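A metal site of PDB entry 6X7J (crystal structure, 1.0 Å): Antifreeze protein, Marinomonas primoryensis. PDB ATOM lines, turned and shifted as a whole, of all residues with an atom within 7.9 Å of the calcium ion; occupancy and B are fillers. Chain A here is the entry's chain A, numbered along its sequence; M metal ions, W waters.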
ATOM      1  N   THR A  15      13.551  -8.973  14.929  1.00  0.00           N
ATOM      2  CA  THR A  15      13.664  -8.352  16.263  1.00  0.00           C
ATOM      3  C   THR A  15      14.896  -7.444  16.260  1.00  0.00           C
ATOM      4  O   THR A  15      15.821  -7.636  15.477  1.00  0.00           O
ATOM      5  CB  THR A  15      13.774  -9.445  17.356  1.00  0.00           C
ATOM      6  OG1 THR A  15      13.833  -8.845  18.660  1.00  0.00           O
ATOM      7  CG2 THR A  15      15.006 -10.310  17.235  1.00  0.00           C
ATOM      8  N   ASN A  16      14.903  -6.488  17.207  1.00  0.00           N
ATOM      9  CA  ASN A  16      16.082  -5.657  17.459  1.00  0.00           C
ATOM     10  C   ASN A  16      16.810  -6.061  18.732  1.00  0.00           C
ATOM     11  O   ASN A  16      17.734  -5.353  19.185  1.00  0.00           O
ATOM     12  CB  ASN A  16      15.709  -4.168  17.433  1.00  0.00           C
ATOM     13  CG  ASN A  16      15.090  -3.797  16.106  1.00  0.00           C
ATOM     14  OD1 ASN A  16      15.572  -4.222  15.051  1.00  0.00           O
ATOM     15  ND2 ASN A  16      14.020  -3.028  16.145  1.00  0.00           N
ATOM     16  N   SER A  17      16.429  -7.199  19.288  1.00  0.00           N
ATOM     17  CA  SER A  17      17.158  -7.878  20.360  1.00  0.00           C
ATOM     18  C   SER A  17      18.106  -8.921  19.764  1.00  0.00           C
ATOM     19  O   SER A  17      17.941  -9.337  18.610  1.00  0.00           O
ATOM     20  CB  SER A  17      16.177  -8.504  21.319  1.00  0.00           C
ATOM     21  OG  SER A  17      15.519  -9.659  20.770  1.00  0.00           O
ATOM     22  N   GLN A  18      19.051  -9.365  20.592  1.00  0.00           N
ATOM     23  CA  GLN A  18      20.017 -10.359  20.130  1.00  0.00           C
ATOM     24  C   GLN A  18      19.396 -11.763  20.214  1.00  0.00           C
ATOM     25  O   GLN A  18      18.892 -12.182  21.252  1.00  0.00           O
ATOM     26  CB  GLN A  18      21.280 -10.310  20.989  1.00  0.00           C
ATOM     27  CG  GLN A  18      22.278 -11.457  20.779  1.00  0.00           C
ATOM     28  CD  GLN A  18      22.969 -11.492  19.436  1.00  0.00           C
ATOM     29  OE1 GLN A  18      22.572 -10.805  18.478  1.00  0.00           O
ATOM     30  NE2 GLN A  18      23.983 -12.326  19.302  1.00  0.00           N
ATOM     31  N   LEU A  19      19.572 -12.526  19.133  1.00  0.00           N
ATOM     32  CA  LEU A  19      19.248 -13.965  19.125  1.00  0.00           C
ATOM     33  C   LEU A  19      20.533 -14.737  19.344  1.00  0.00           C
ATOM     34  O   LEU A  19      21.432 -14.708  18.498  1.00  0.00           O
ATOM     35  CB  LEU A  19      18.600 -14.334  17.792  1.00  0.00           C
ATOM     36  CG  LEU A  19      17.262 -13.659  17.516  1.00  0.00           C
ATOM     37  CD1 LEU A  19      16.778 -14.018  16.109  1.00  0.00           C
ATOM     38  CD2 LEU A  19      16.216 -14.054  18.533  1.00  0.00           C
ATOM     39  N   ASN A  20      20.653 -15.434  20.474  1.00  0.00           N
ATOM     40  CA  ASN A  20      21.844 -16.241  20.813  1.00  0.00           C
ATOM     41  C   ASN A  20      21.640 -17.749  20.667  1.00  0.00           C
ATOM     42  O   ASN A  20      22.635 -18.478  20.657  1.00  0.00           O
ATOM     43  CB  ASN A  20      22.344 -15.950  22.231  1.00  0.00           C
ATOM     44  CG  ASN A  20      23.029 -14.597  22.374  1.00  0.00           C
ATOM     45  OD1 ASN A  20      23.909 -14.276  21.567  1.00  0.00           O
ATOM     46  ND2 ASN A  20      22.624 -13.801  23.359  1.00  0.00           N
ATOM     47  N   ASP A  51      23.047  -8.892   7.028  1.00  0.00           N
ATOM     48  CA  ASP A  51      21.935  -9.136   7.959  1.00  0.00           C
ATOM     49  C   ASP A  51      20.655  -9.572   7.217  1.00  0.00           C
ATOM     50  O   ASP A  51      20.097  -8.834   6.373  1.00  0.00           O
ATOM     51  CB  ASP A  51      21.554  -7.879   8.787  1.00  0.00           C
ATOM     52  CG  ASP A  51      22.703  -7.235   9.497  1.00  0.00           C
ATOM     53  OD1 ASP A  51      23.625  -7.889   9.946  1.00  0.00           O
ATOM     54  OD2 ASP A  51      22.540  -6.008   9.769  1.00  0.00           O
ATOM     55  N   THR A  77      17.407  -5.901  13.251  1.00  0.00           N
ATOM     56  CA  THR A  77      18.816  -6.334  13.325  1.00  0.00           C
ATOM     57  C   THR A  77      18.951  -7.837  13.171  1.00  0.00           C
ATOM     58  O   THR A  77      19.966  -8.318  12.594  1.00  0.00           O
ATOM     59  CB  THR A  77      19.480  -5.850  14.615  1.00  0.00           C
ATOM     60  OG1 THR A  77      18.926  -6.474  15.773  1.00  0.00           O
ATOM     61  CG2 THR A  77      19.346  -4.342  14.800  1.00  0.00           C
ATOM     62  N   ASP A  78      18.009  -8.602  13.720  1.00  0.00           N
ATOM     63  CA  ASP A  78      18.076 -10.056  13.842  1.00  0.00           C
ATOM     64  C   ASP A  78      16.789 -10.625  13.308  1.00  0.00           C
ATOM     65  O   ASP A  78      15.722  -9.961  13.381  1.00  0.00           O
ATOM     66  CB  ASP A  78      18.242 -10.464  15.326  1.00  0.00           C
ATOM     67  CG  ASP A  78      19.583 -10.093  15.973  1.00  0.00           C
ATOM     68  OD1 ASP A  78      20.014  -8.909  15.835  1.00  0.00           O
ATOM     69  OD2 ASP A  78      20.223 -10.948  16.606  1.00  0.00           O
ATOM     70  N   GLY A  79      16.778 -11.856  12.829  1.00  0.00           N
ATOM     71  CA  GLY A  79      15.528 -12.433  12.392  1.00  0.00           C
ATOM     72  C   GLY A  79      15.679 -13.914  12.084  1.00  0.00           C
ATOM     73  O   GLY A  79      16.786 -14.422  12.004  1.00  0.00           O
ATOM     74  N   ASP A 102      22.863 -18.578  11.181  1.00  0.00           N
ATOM     75  CA  ASP A 102      23.442 -18.984  12.455  1.00  0.00           C
ATOM     76  C   ASP A 102      22.955 -20.405  12.810  1.00  0.00           C
ATOM     77  O   ASP A 102      23.289 -21.345  12.059  1.00  0.00           O
ATOM     78  CB  ASP A 102      23.173 -17.905  13.521  1.00  0.00           C
ATOM     79  CG  ASP A 102      24.099 -16.726  13.308  1.00  0.00           C
ATOM     80  OD1 ASP A 102      25.266 -16.816  13.766  1.00  0.00           O
ATOM     81  OD2 ASP A 102      23.679 -15.711  12.666  1.00  0.00           O
ATOM     82  N   ASN A 119      25.088 -19.458  17.899  1.00  0.00           N
ATOM     83  CA  ASN A 119      25.465 -18.713  16.702  1.00  0.00           C
ATOM     84  C   ASN A 119      26.725 -19.294  16.090  1.00  0.00           C
ATOM     85  O   ASN A 119      27.547 -19.933  16.758  1.00  0.00           O
ATOM     86  CB  ASN A 119      25.628 -17.250  17.049  1.00  0.00           C
ATOM     87  CG  ASN A 119      24.294 -16.615  17.349  1.00  0.00           C
ATOM     88  OD1 ASN A 119      23.285 -17.002  16.789  1.00  0.00           O
ATOM     89  ND2 ASN A 119      24.282 -15.590  18.189  1.00  0.00           N
ATOM     90  N   TRP A 145      17.798 -19.052  12.477  1.00  0.00           N
ATOM     91  CA  TRP A 145      17.876 -17.585  12.626  1.00  0.00           C
ATOM     92  C   TRP A 145      19.227 -17.083  12.223  1.00  0.00           C
ATOM     93  O   TRP A 145      20.216 -17.823  12.109  1.00  0.00           O
ATOM     94  CB  TRP A 145      17.531 -17.152  14.075  1.00  0.00           C
ATOM     95  CG  TRP A 145      18.629 -17.461  15.056  1.00  0.00           C
ATOM     96  CD1 TRP A 145      19.670 -16.643  15.396  1.00  0.00           C
ATOM     97  CD2 TRP A 145      18.890 -18.708  15.724  1.00  0.00           C
ATOM     98  NE1 TRP A 145      20.550 -17.262  16.246  1.00  0.00           N
ATOM     99  CE2 TRP A 145      20.124 -18.540  16.425  1.00  0.00           C
ATOM    100  CE3 TRP A 145      18.229 -19.925  15.792  1.00  0.00           C
ATOM    101  CZ2 TRP A 145      20.693 -19.571  17.179  1.00  0.00           C
ATOM    102  CZ3 TRP A 145      18.796 -20.943  16.511  1.00  0.00           C
ATOM    103  CH2 TRP A 145      20.029 -20.771  17.179  1.00  0.00           C
ATOM    104  N   ASP A 146      19.250 -15.755  12.053  1.00  0.00           N
ATOM    105  CA  ASP A 146      20.453 -14.944  11.831  1.00  0.00           C
ATOM    106  C   ASP A 146      20.542 -13.909  12.937  1.00  0.00           C
ATOM    107  O   ASP A 146      19.629 -13.105  13.139  1.00  0.00           O
ATOM    108  CB  ASP A 146      20.385 -14.237  10.472  1.00  0.00           C
ATOM    109  CG  ASP A 146      21.563 -13.296  10.241  1.00  0.00           C
ATOM    110  OD1 ASP A 146      22.680 -13.672  10.673  1.00  0.00           O
ATOM    111  OD2 ASP A 146      21.359 -12.185   9.692  1.00  0.00           O
ATOM    112  N   GLN A 147      21.660 -13.919  13.667  1.00  0.00           N
ATOM    113  CA  GLN A 147      21.955 -12.893  14.698  1.00  0.00           C
ATOM    114  C   GLN A 147      22.556 -11.637  14.076  1.00  0.00           C
ATOM    115  O   GLN A 147      22.750 -10.643  14.781  1.00  0.00           O
ATOM    116  CB  GLN A 147      22.904 -13.454  15.760  1.00  0.00           C
ATOM    117  CG  GLN A 147      24.345 -13.693  15.297  1.00  0.00           C
ATOM    118  CD  GLN A 147      25.267 -12.539  15.528  1.00  0.00           C
ATOM    119  OE1 GLN A 147      25.307 -11.968  16.638  1.00  0.00           O
ATOM    120  NE2 GLN A 147      26.028 -12.145  14.519  1.00  0.00           N
ATOM    121  N   GLY A 148      22.909 -11.688  12.798  1.00  0.00           N
ATOM    122  CA  GLY A 148      23.557 -10.597  12.098  1.00  0.00           C
ATOM    123  C   GLY A 148      24.640 -11.118  11.189  1.00  0.00           C
ATOM    124  O   GLY A 148      25.177 -12.234  11.375  1.00  0.00           O
ATOM    125  N   GLY A 149      25.006 -10.289  10.218  1.00  0.00           N
ATOM    126  CA  GLY A 149      26.107 -10.584   9.305  1.00  0.00           C
ATOM    127  C   GLY A 149      25.696 -11.487   8.170  1.00  0.00           C
ATOM    128  O   GLY A 149      24.754 -11.158   7.432  1.00  0.00           O
HETATM  129 CA    CA M   1      22.218  -9.409  16.685  1.00  0.00          CA
HETATM  130  O   HOH W   1      21.842  -7.900  18.469  1.00  0.00           O
HETATM  131  O   HOH W   2      24.657  -9.317  16.865  1.00  0.00           O
HETATM  132  O   HOH W   3      22.865  -7.435  15.489  1.00  0.00           O
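The side-chain amide nitrogen of Gln 18 lies close to the side-chain amide nitrogen of Asn 119, 3.5 Å away. OD1 of Asn 20 sits at hydrogen-bond distance from NE2 of Gln 18 (3.0 Å). The backbone NH (N) of Gln 147 lies close to the side-chain carboxylate (OD2) of Asp 102. OG1 of Thr 77 lies close to OD1 of Asp 78 (2.7 Å). The side-chain carboxylate (OD2) of Asp 78 lies close to the backbone NH (N) of Leu 19 (3.0 Å). The backbone carbonyl oxygen of Asp 78 sits at hydrogen-bond distance from the backbone NH of Thr 15, 2.8 Å away.
The calcium ion is bound by the side-chain amide oxygen (OE1) of Gln 18, the backbone carbonyl oxygen (O) of Gln 147, water W1, water W3, the side-chain carboxylate (OD1) of Asp 78, water W2 and the side-chain carboxylate (OD2) of Asp 78. The calcium ion has seven donor atoms within binding distance.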
